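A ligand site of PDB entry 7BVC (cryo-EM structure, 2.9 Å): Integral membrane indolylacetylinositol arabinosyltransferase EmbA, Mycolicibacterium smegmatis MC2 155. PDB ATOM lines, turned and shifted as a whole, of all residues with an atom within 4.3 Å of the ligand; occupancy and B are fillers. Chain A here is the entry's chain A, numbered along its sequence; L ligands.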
ATOM      1  N   ASP A 269      -6.837  -0.724 -30.568  1.00  0.00           N
ATOM      2  CA  ASP A 269      -5.551  -0.124 -30.902  1.00  0.00           C
ATOM      3  C   ASP A 269      -4.631  -1.084 -31.643  1.00  0.00           C
ATOM      4  O   ASP A 269      -3.418  -1.094 -31.423  1.00  0.00           O
ATOM      5  CB  ASP A 269      -4.872   0.399 -29.639  1.00  0.00           C
ATOM      6  CG  ASP A 269      -5.724   1.411 -28.895  1.00  0.00           C
ATOM      7  OD1 ASP A 269      -6.083   2.438 -29.503  1.00  0.00           O
ATOM      8  OD2 ASP A 269      -6.036   1.164 -27.706  1.00  0.00           O
ATOM      9  N   TYR A 272      -3.724   1.079 -35.057  1.00  0.00           N
ATOM     10  CA  TYR A 272      -2.897   2.219 -34.695  1.00  0.00           C
ATOM     11  C   TYR A 272      -1.436   1.800 -34.539  1.00  0.00           C
ATOM     12  O   TYR A 272      -0.534   2.321 -35.221  1.00  0.00           O
ATOM     13  CB  TYR A 272      -3.426   2.838 -33.404  1.00  0.00           C
ATOM     14  CG  TYR A 272      -2.760   4.110 -32.958  1.00  0.00           C
ATOM     15  CD1 TYR A 272      -3.063   5.322 -33.564  1.00  0.00           C
ATOM     16  CD2 TYR A 272      -1.841   4.108 -31.936  1.00  0.00           C
ATOM     17  CE1 TYR A 272      -2.463   6.490 -33.166  1.00  0.00           C
ATOM     18  CE2 TYR A 272      -1.223   5.273 -31.523  1.00  0.00           C
ATOM     19  CZ  TYR A 272      -1.551   6.457 -32.147  1.00  0.00           C
ATOM     20  OH  TYR A 272      -0.942   7.624 -31.730  1.00  0.00           O
ATOM     21  N   ASN A 273      -1.186   0.833 -33.652  1.00  0.00           N
ATOM     22  CA  ASN A 273       0.187   0.376 -33.409  1.00  0.00           C
ATOM     23  C   ASN A 273       0.775  -0.310 -34.629  1.00  0.00           C
ATOM     24  O   ASN A 273       1.980  -0.212 -34.861  1.00  0.00           O
ATOM     25  CB  ASN A 273       0.202  -0.563 -32.214  1.00  0.00           C
ATOM     26  CG  ASN A 273      -0.336   0.085 -30.951  1.00  0.00           C
ATOM     27  OD1 ASN A 273      -0.183   1.284 -30.749  1.00  0.00           O
ATOM     28  ND2 ASN A 273      -0.981  -0.710 -30.118  1.00  0.00           N
ATOM     29  N   GLU A 297       6.627   9.311 -30.053  1.00  0.00           N
ATOM     30  CA  GLU A 297       6.198   8.529 -28.892  1.00  0.00           C
ATOM     31  C   GLU A 297       7.317   8.436 -27.870  1.00  0.00           C
ATOM     32  O   GLU A 297       7.668   7.366 -27.395  1.00  0.00           O
ATOM     33  CB  GLU A 297       5.750   7.136 -29.338  1.00  0.00           C
ATOM     34  CG  GLU A 297       4.592   7.133 -30.316  1.00  0.00           C
ATOM     35  CD  GLU A 297       3.267   7.494 -29.672  1.00  0.00           C
ATOM     36  OE1 GLU A 297       3.074   7.142 -28.484  1.00  0.00           O
ATOM     37  OE2 GLU A 297       2.437   8.130 -30.337  1.00  0.00           O
ATOM     38  N   PHE A 300       7.502   6.328 -24.382  1.00  0.00           N
ATOM     39  CA  PHE A 300       6.783   5.059 -24.335  1.00  0.00           C
ATOM     40  C   PHE A 300       6.883   4.313 -25.664  1.00  0.00           C
ATOM     41  O   PHE A 300       5.872   3.869 -26.225  1.00  0.00           O
ATOM     42  CB  PHE A 300       5.321   5.278 -23.956  1.00  0.00           C
ATOM     43  CG  PHE A 300       5.137   5.982 -22.643  1.00  0.00           C
ATOM     44  CD1 PHE A 300       5.808   5.543 -21.511  1.00  0.00           C
ATOM     45  CD2 PHE A 300       4.301   7.072 -22.538  1.00  0.00           C
ATOM     46  CE1 PHE A 300       5.643   6.193 -20.300  1.00  0.00           C
ATOM     47  CE2 PHE A 300       4.136   7.722 -21.326  1.00  0.00           C
ATOM     48  CZ  PHE A 300       4.800   7.278 -20.207  1.00  0.00           C
ATOM     49  N   GLN A 304       7.104  -0.445 -29.617  1.00  0.00           N
ATOM     50  CA  GLN A 304       6.942  -0.195 -31.044  1.00  0.00           C
ATOM     51  C   GLN A 304       8.236  -0.459 -31.801  1.00  0.00           C
ATOM     52  O   GLN A 304       8.193  -0.816 -32.987  1.00  0.00           O
ATOM     53  CB  GLN A 304       6.463   1.232 -31.289  1.00  0.00           C
ATOM     54  CG  GLN A 304       4.957   1.370 -31.348  1.00  0.00           C
ATOM     55  CD  GLN A 304       4.345   1.661 -29.999  1.00  0.00           C
ATOM     56  OE1 GLN A 304       5.049   2.036 -29.058  1.00  0.00           O
ATOM     57  NE2 GLN A 304       3.041   1.480 -29.887  1.00  0.00           N
ATOM     58  N   ARG A 373      -1.485  -4.116 -27.761  1.00  0.00           N
ATOM     59  CA  ARG A 373      -1.371  -3.183 -26.654  1.00  0.00           C
ATOM     60  C   ARG A 373      -0.351  -3.687 -25.641  1.00  0.00           C
ATOM     61  O   ARG A 373      -0.016  -4.873 -25.625  1.00  0.00           O
ATOM     62  CB  ARG A 373      -2.742  -3.009 -25.993  1.00  0.00           C
ATOM     63  CG  ARG A 373      -3.697  -2.157 -26.798  1.00  0.00           C
ATOM     64  CD  ARG A 373      -4.972  -1.882 -26.029  1.00  0.00           C
ATOM     65  NE  ARG A 373      -4.706  -1.237 -24.748  1.00  0.00           N
ATOM     66  CZ  ARG A 373      -4.983   0.033 -24.477  1.00  0.00           C
ATOM     67  NH1 ARG A 373      -5.535   0.812 -25.403  1.00  0.00           N
ATOM     68  NH2 ARG A 373      -4.706   0.538 -23.285  1.00  0.00           N
ATOM     69  N   PRO A 374       0.169  -2.817 -24.785  1.00  0.00           N
ATOM     70  CA  PRO A 374       1.169  -3.245 -23.792  1.00  0.00           C
ATOM     71  C   PRO A 374       0.604  -3.880 -22.524  1.00  0.00           C
ATOM     72  O   PRO A 374       1.385  -4.253 -21.645  1.00  0.00           O
ATOM     73  CB  PRO A 374       1.870  -1.918 -23.451  1.00  0.00           C
ATOM     74  CG  PRO A 374       0.814  -0.899 -23.621  1.00  0.00           C
ATOM     75  CD  PRO A 374       0.022  -1.348 -24.818  1.00  0.00           C
ATOM     76  N   MET A 409      11.128  -1.209 -14.103  1.00  0.00           N
ATOM     77  CA  MET A 409      11.487  -0.059 -14.928  1.00  0.00           C
ATOM     78  C   MET A 409      11.221  -0.328 -16.403  1.00  0.00           C
ATOM     79  O   MET A 409      10.898   0.595 -17.150  1.00  0.00           O
ATOM     80  CB  MET A 409      12.961   0.296 -14.720  1.00  0.00           C
ATOM     81  CG  MET A 409      13.264   0.874 -13.346  1.00  0.00           C
ATOM     82  SD  MET A 409      12.168   2.223 -12.881  1.00  0.00           S
ATOM     83  CE  MET A 409      11.419   1.559 -11.407  1.00  0.00           C
ATOM     84  N   PRO A 416       1.662   4.801 -19.609  1.00  0.00           N
ATOM     85  CA  PRO A 416       1.459   5.508 -18.335  1.00  0.00           C
ATOM     86  C   PRO A 416       0.824   4.649 -17.260  1.00  0.00           C
ATOM     87  O   PRO A 416       1.191   4.754 -16.086  1.00  0.00           O
ATOM     88  CB  PRO A 416       0.561   6.682 -18.735  1.00  0.00           C
ATOM     89  CG  PRO A 416       0.852   6.913 -20.159  1.00  0.00           C
ATOM     90  CD  PRO A 416       1.141   5.561 -20.757  1.00  0.00           C
ATOM     91  N   GLN A 417      -0.124   3.788 -17.641  1.00  0.00           N
ATOM     92  CA  GLN A 417      -0.765   2.899 -16.680  1.00  0.00           C
ATOM     93  C   GLN A 417       0.125   1.741 -16.255  1.00  0.00           C
ATOM     94  O   GLN A 417      -0.319   0.889 -15.476  1.00  0.00           O
ATOM     95  CB  GLN A 417      -2.075   2.350 -17.257  1.00  0.00           C
ATOM     96  CG  GLN A 417      -1.891   1.236 -18.274  1.00  0.00           C
ATOM     97  CD  GLN A 417      -2.011   1.724 -19.699  1.00  0.00           C
ATOM     98  OE1 GLN A 417      -1.857   2.902 -19.979  1.00  0.00           O
ATOM     99  NE2 GLN A 417      -2.288   0.795 -20.615  1.00  0.00           N
ATOM    100  N   LEU A 419       2.710   1.890 -14.336  1.00  0.00           N
ATOM    101  CA  LEU A 419       3.366   2.127 -13.063  1.00  0.00           C
ATOM    102  C   LEU A 419       2.826   1.248 -11.952  1.00  0.00           C
ATOM    103  O   LEU A 419       3.373   1.277 -10.847  1.00  0.00           O
ATOM    104  CB  LEU A 419       3.229   3.595 -12.655  1.00  0.00           C
ATOM    105  CG  LEU A 419       1.916   4.077 -12.031  1.00  0.00           C
ATOM    106  CD1 LEU A 419       2.123   5.415 -11.347  1.00  0.00           C
ATOM    107  CD2 LEU A 419       0.797   4.157 -13.048  1.00  0.00           C
ATOM    108  N   VAL A 456      17.491   1.375 -10.755  1.00  0.00           N
ATOM    109  CA  VAL A 456      16.549   2.435 -11.070  1.00  0.00           C
ATOM    110  C   VAL A 456      17.123   3.372 -12.135  1.00  0.00           C
ATOM    111  O   VAL A 456      16.369   4.026 -12.857  1.00  0.00           O
ATOM    112  CB  VAL A 456      16.175   3.211  -9.797  1.00  0.00           C
ATOM    113  CG1 VAL A 456      15.123   4.281 -10.086  1.00  0.00           C
ATOM    114  CG2 VAL A 456      15.689   2.264  -8.712  1.00  0.00           C
ATOM    115  N   PHE A 460      16.885   5.968 -17.741  1.00  0.00           N
ATOM    116  CA  PHE A 460      17.552   7.016 -18.506  1.00  0.00           C
ATOM    117  C   PHE A 460      18.257   6.464 -19.741  1.00  0.00           C
ATOM    118  O   PHE A 460      18.493   7.218 -20.693  1.00  0.00           O
ATOM    119  CB  PHE A 460      18.532   7.771 -17.622  1.00  0.00           C
ATOM    120  CG  PHE A 460      17.891   8.406 -16.423  1.00  0.00           C
ATOM    121  CD1 PHE A 460      16.944   9.408 -16.573  1.00  0.00           C
ATOM    122  CD2 PHE A 460      18.227   8.011 -15.142  1.00  0.00           C
ATOM    123  CE1 PHE A 460      16.351   9.993 -15.487  1.00  0.00           C
ATOM    124  CE2 PHE A 460      17.640   8.599 -14.043  1.00  0.00           C
ATOM    125  CZ  PHE A 460      16.692   9.587 -14.213  1.00  0.00           C
ATOM    126  N   VAL A 476       6.057  15.632 -24.871  1.00  0.00           N
ATOM    127  CA  VAL A 476       5.085  15.585 -23.776  1.00  0.00           C
ATOM    128  C   VAL A 476       4.272  16.868 -23.737  1.00  0.00           C
ATOM    129  O   VAL A 476       3.064  16.848 -23.493  1.00  0.00           O
ATOM    130  CB  VAL A 476       5.801  15.328 -22.441  1.00  0.00           C
ATOM    131  CG1 VAL A 476       4.809  15.349 -21.298  1.00  0.00           C
ATOM    132  CG2 VAL A 476       6.528  13.995 -22.476  1.00  0.00           C
ATOM    133  N   LYS A 479       1.647  16.680 -26.479  1.00  0.00           N
ATOM    134  CA  LYS A 479       0.596  15.730 -26.143  1.00  0.00           C
ATOM    135  C   LYS A 479      -0.303  16.251 -25.033  1.00  0.00           C
ATOM    136  O   LYS A 479      -1.481  15.864 -24.961  1.00  0.00           O
ATOM    137  CB  LYS A 479       1.199  14.386 -25.750  1.00  0.00           C
ATOM    138  CG  LYS A 479       1.861  13.649 -26.895  1.00  0.00           C
ATOM    139  CD  LYS A 479       1.534  12.166 -26.851  1.00  0.00           C
ATOM    140  CE  LYS A 479       2.339  11.390 -27.879  1.00  0.00           C
ATOM    141  NZ  LYS A 479       3.795  11.581 -27.675  1.00  0.00           N
ATOM    142  N   TYR A 480       0.219  17.108 -24.148  1.00  0.00           N
ATOM    143  CA  TYR A 480      -0.622  17.650 -23.086  1.00  0.00           C
ATOM    144  C   TYR A 480      -1.436  18.859 -23.535  1.00  0.00           C
ATOM    145  O   TYR A 480      -2.559  19.052 -23.063  1.00  0.00           O
ATOM    146  CB  TYR A 480       0.223  18.023 -21.870  1.00  0.00           C
ATOM    147  CG  TYR A 480       0.221  16.975 -20.782  1.00  0.00           C
ATOM    148  CD1 TYR A 480      -0.829  16.886 -19.891  1.00  0.00           C
ATOM    149  CD2 TYR A 480       1.259  16.066 -20.662  1.00  0.00           C
ATOM    150  CE1 TYR A 480      -0.839  15.928 -18.894  1.00  0.00           C
ATOM    151  CE2 TYR A 480       1.258  15.107 -19.670  1.00  0.00           C
ATOM    152  CZ  TYR A 480       0.202  15.041 -18.800  1.00  0.00           C
ATOM    153  OH  TYR A 480       0.192  14.083 -17.802  1.00  0.00           O
ATOM    154  N   LEU A 558      -3.300   8.646 -11.343  1.00  0.00           N
ATOM    155  CA  LEU A 558      -2.365   9.585 -11.948  1.00  0.00           C
ATOM    156  C   LEU A 558      -2.231   9.428 -13.456  1.00  0.00           C
ATOM    157  O   LEU A 558      -1.470  10.187 -14.074  1.00  0.00           O
ATOM    158  CB  LEU A 558      -0.987   9.446 -11.293  1.00  0.00           C
ATOM    159  CG  LEU A 558      -0.970   9.171  -9.785  1.00  0.00           C
ATOM    160  CD1 LEU A 558       0.445   8.908  -9.306  1.00  0.00           C
ATOM    161  CD2 LEU A 558      -1.582  10.335  -9.022  1.00  0.00           C
ATOM    162  N   PRO A 560      -3.143   9.802 -17.420  1.00  0.00           N
ATOM    163  CA  PRO A 560      -3.840  10.862 -18.167  1.00  0.00           C
ATOM    164  C   PRO A 560      -5.109  10.371 -18.862  1.00  0.00           C
ATOM    165  O   PRO A 560      -6.091  11.113 -18.969  1.00  0.00           O
ATOM    166  CB  PRO A 560      -2.801  11.327 -19.186  1.00  0.00           C
ATOM    167  CG  PRO A 560      -1.495  10.708 -18.753  1.00  0.00           C
ATOM    168  CD  PRO A 560      -1.866   9.453 -18.049  1.00  0.00           C
ATOM    169  N   THR A 561      -5.092   9.134 -19.341  1.00  0.00           N
ATOM    170  CA  THR A 561      -6.234   8.537 -20.016  1.00  0.00           C
ATOM    171  C   THR A 561      -6.808   7.422 -19.157  1.00  0.00           C
ATOM    172  O   THR A 561      -6.064   6.664 -18.531  1.00  0.00           O
ATOM    173  CB  THR A 561      -5.846   7.983 -21.383  1.00  0.00           C
ATOM    174  OG1 THR A 561      -4.589   7.301 -21.290  1.00  0.00           O
ATOM    175  CG2 THR A 561      -5.720   9.121 -22.393  1.00  0.00           C
ATOM    176  N   TRP A 563      -9.528   5.010 -20.011  1.00  0.00           N
ATOM    177  CA  TRP A 563     -10.448   4.114 -20.708  1.00  0.00           C
ATOM    178  C   TRP A 563     -10.756   2.893 -19.848  1.00  0.00           C
ATOM    179  O   TRP A 563     -10.166   2.687 -18.778  1.00  0.00           O
ATOM    180  CB  TRP A 563      -9.857   3.691 -22.055  1.00  0.00           C
ATOM    181  CG  TRP A 563      -9.275   4.810 -22.853  1.00  0.00           C
ATOM    182  CD1 TRP A 563      -7.991   4.922 -23.294  1.00  0.00           C
ATOM    183  CD2 TRP A 563      -9.965   5.971 -23.333  1.00  0.00           C
ATOM    184  NE1 TRP A 563      -7.832   6.076 -23.999  1.00  0.00           N
ATOM    185  CE2 TRP A 563      -9.030   6.745 -24.037  1.00  0.00           C
ATOM    186  CE3 TRP A 563     -11.278   6.445 -23.219  1.00  0.00           C
ATOM    187  CZ2 TRP A 563      -9.362   7.954 -24.633  1.00  0.00           C
ATOM    188  CZ3 TRP A 563     -11.602   7.638 -23.816  1.00  0.00           C
ATOM    189  CH2 TRP A 563     -10.652   8.388 -24.503  1.00  0.00           C
ATOM    190  N   GLN A 566      -8.069  -0.495 -19.948  1.00  0.00           N
ATOM    191  CA  GLN A 566      -6.842  -0.517 -19.162  1.00  0.00           C
ATOM    192  C   GLN A 566      -6.939  -1.414 -17.933  1.00  0.00           C
ATOM    193  O   GLN A 566      -5.958  -1.524 -17.198  1.00  0.00           O
ATOM    194  CB  GLN A 566      -6.467   0.901 -18.733  1.00  0.00           C
ATOM    195  CG  GLN A 566      -6.364   1.881 -19.890  1.00  0.00           C
ATOM    196  CD  GLN A 566      -6.004   3.270 -19.435  1.00  0.00           C
ATOM    197  OE1 GLN A 566      -5.923   3.549 -18.238  1.00  0.00           O
ATOM    198  NE2 GLN A 566      -5.782   4.163 -20.397  1.00  0.00           N
ATOM    199  N   ASN A 788     -10.792   6.238 -29.298  1.00  0.00           N
ATOM    200  CA  ASN A 788     -10.154   7.210 -30.183  1.00  0.00           C
ATOM    201  C   ASN A 788     -11.163   8.293 -30.592  1.00  0.00           C
ATOM    202  O   ASN A 788     -11.547   8.431 -31.749  1.00  0.00           O
ATOM    203  CB  ASN A 788      -9.555   6.517 -31.398  1.00  0.00           C
ATOM    204  CG  ASN A 788      -8.271   5.787 -31.061  1.00  0.00           C
ATOM    205  OD1 ASN A 788      -7.581   6.134 -30.094  1.00  0.00           O
ATOM    206  ND2 ASN A 788      -7.931   4.793 -31.859  1.00  0.00           N
HETATM  207  C1  LIG L   1      13.295  10.041 -11.451  1.00  0.00           C
HETATM  208  C2  LIG L   1      13.994   8.675 -11.173  1.00  0.00           C
HETATM  209  C3  LIG L   1      15.395   8.649 -10.534  1.00  0.00           C
HETATM  210  C4  LIG L   1      13.380   7.511 -11.488  1.00  0.00           C
HETATM  211  C5  LIG L   1      11.973   7.733 -12.118  1.00  0.00           C
HETATM  212  C6  LIG L   1      11.258   6.371 -12.364  1.00  0.00           C
HETATM  213  C7  LIG L   1      10.405   5.990 -11.122  1.00  0.00           C
HETATM  214  C8  LIG L   1      11.073   5.308  -9.913  1.00  0.00           C
HETATM  215  C9  LIG L   1       9.073   6.248 -11.082  1.00  0.00           C
HETATM  216  C10 LIG L   1       8.542   6.937 -12.379  1.00  0.00           C
HETATM  217  C11 LIG L   1       6.996   7.104 -12.282  1.00  0.00           C
HETATM  218  C12 LIG L   1       6.462   7.785 -13.583  1.00  0.00           C
HETATM  219  C13 LIG L   1       7.447   8.564 -14.502  1.00  0.00           C
HETATM  220  C14 LIG L   1       5.152   7.686 -13.890  1.00  0.00           C
HETATM  221  C15 LIG L   1       4.784   8.416 -15.216  1.00  0.00           C
HETATM  222  C16 LIG L   1       3.315   8.073 -15.618  1.00  0.00           C
HETATM  223  C17 LIG L   1       2.342   9.138 -15.040  1.00  0.00           C
HETATM  224  C18 LIG L   1       1.885   9.030 -13.560  1.00  0.00           C
HETATM  225  C19 LIG L   1       1.879  10.160 -15.806  1.00  0.00           C
HETATM  226  C20 LIG L   1       2.432  10.103 -17.263  1.00  0.00           C
HETATM  227  C21 LIG L   1       3.444  11.276 -17.462  1.00  0.00           C
HETATM  228  C22 LIG L   1       3.484  11.664 -18.962  1.00  0.00           C
HETATM  229  C23 LIG L   1       4.843  11.976 -19.634  1.00  0.00           C
HETATM  230  C24 LIG L   1       2.328  11.712 -19.663  1.00  0.00           C
HETATM  231  C25 LIG L   1       2.535  12.109 -21.151  1.00  0.00           C
HETATM  232  C26 LIG L   1       1.136  12.283 -21.838  1.00  0.00           C
HETATM  233  C27 LIG L   1       0.964  11.157 -22.903  1.00  0.00           C
HETATM  234  C28 LIG L   1       2.212  10.558 -23.571  1.00  0.00           C
HETATM  235  C29 LIG L   1      -0.276  10.725 -23.203  1.00  0.00           C
HETATM  236  C30 LIG L   1      -0.278   9.604 -24.272  1.00  0.00           C
HETATM  237  C31 LIG L   1      -1.011   8.354 -23.701  1.00  0.00           C
HETATM  238  C32 LIG L   1      -0.179   7.078 -24.016  1.00  0.00           C
HETATM  239  C33 LIG L   1       1.206   7.205 -24.686  1.00  0.00           C
HETATM  240  C34 LIG L   1      -0.648   5.857 -23.695  1.00  0.00           C
HETATM  241  C35 LIG L   1      -2.046   5.896 -23.019  1.00  0.00           C
HETATM  242  C36 LIG L   1      -1.873   3.551 -25.908  1.00  0.00           C
HETATM  243  C37 LIG L   1      -1.502   2.609 -26.773  1.00  0.00           C
HETATM  244  C38 LIG L   1      -1.518   3.264 -28.275  1.00  0.00           C
HETATM  245  C39 LIG L   1      -2.112   4.486 -28.188  1.00  0.00           C
HETATM  246  C40 LIG L   1      -3.594   4.396 -28.544  1.00  0.00           C
HETATM  247  O1  LIG L   1      -2.611   4.591 -23.056  1.00  0.00           O
HETATM  248  O2  LIG L   1      -4.956   3.630 -23.584  1.00  0.00           O
HETATM  249  O3  LIG L   1      -3.111   3.243 -25.356  1.00  0.00           O
HETATM  250  O4  LIG L   1      -1.961   4.923 -26.727  1.00  0.00           O
HETATM  251  O5  LIG L   1      -2.434   1.510 -26.710  1.00  0.00           O
HETATM  252  O6  LIG L   1      -0.190   3.396 -28.747  1.00  0.00           O
HETATM  253  O7  LIG L   1      -4.123   5.691 -28.576  1.00  0.00           O
HETATM  254  O8  LIG L   1      -4.147   5.566 -24.885  1.00  0.00           O
HETATM  255  P1  LIG L   1      -3.750   4.267 -24.221  1.00  0.00           P
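The side-chain amide nitrogen of Gln 566 lies within hydrogen-bond range of an oxygen (O2) of the ligand. OD1 of Asn 273 is in hydrogen-bond range of O6 of the ligand. An oxygen (O2) of the ligand lies within salt-bridge range of the guanidinium group of Arg 373 (3.1 Å).
O of Thr 561 sits close to OE1 of Gln 566 (3.1 Å). OD1 of Asn 273 sits at hydrogen-bond distance from NE2 of Gln 304 (3.3 Å). The side-chain amide nitrogen (ND2) of Asn 273 sits at hydrogen-bond distance from the backbone carbonyl oxygen (O) of Asp 269, at 2.8 Å. O of Phe 300 lies close to OE1 of Gln 304 (3.5 Å).
OD1 of Asp 269 touches C40 of the ligand, at 3.3 Å. Tyr 272 touches the ligand. Phe 300 touches the ligand (CD2 to C33, 3.8 Å). Gln 304 touches the ligand. Pro 416 touches the ligand. OE1 of Gln 417 touches O1 of the ligand (3.6 Å). CG1 of Val 456 touches C4 of the ligand, at 3.9 Å. CG1 of Val 476 touches C23 of the ligand, at 3.8 Å. CD of Lys 479 touches C28 of the ligand, at 3.7 Å. Tyr 480 touches the ligand (CE2 to C24, 3.6 Å). Leu 558 touches the ligand (O to C18, 3.6 Å). OG1 of Thr 561 touches C35 of the ligand, at 3.4 Å. CD1 of Trp 563 touches O2 of the ligand, 3.3 Å away. OD1 of Asn 788 touches O7 of the ligand, 3.8 Å away. Within 4 Å of the ligand: Asp 269, Tyr 272, Asn 273, Phe 300, Gln 304, Arg 373, Pro 416, Gln 417, Val 456, Val 476, Lys 479, Tyr 480, Leu 558, Thr 561, Trp 563, Gln 566 and Asn 788. The nearest printed residue that does not touch the ligand is Phe 460 (4.01 Å).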
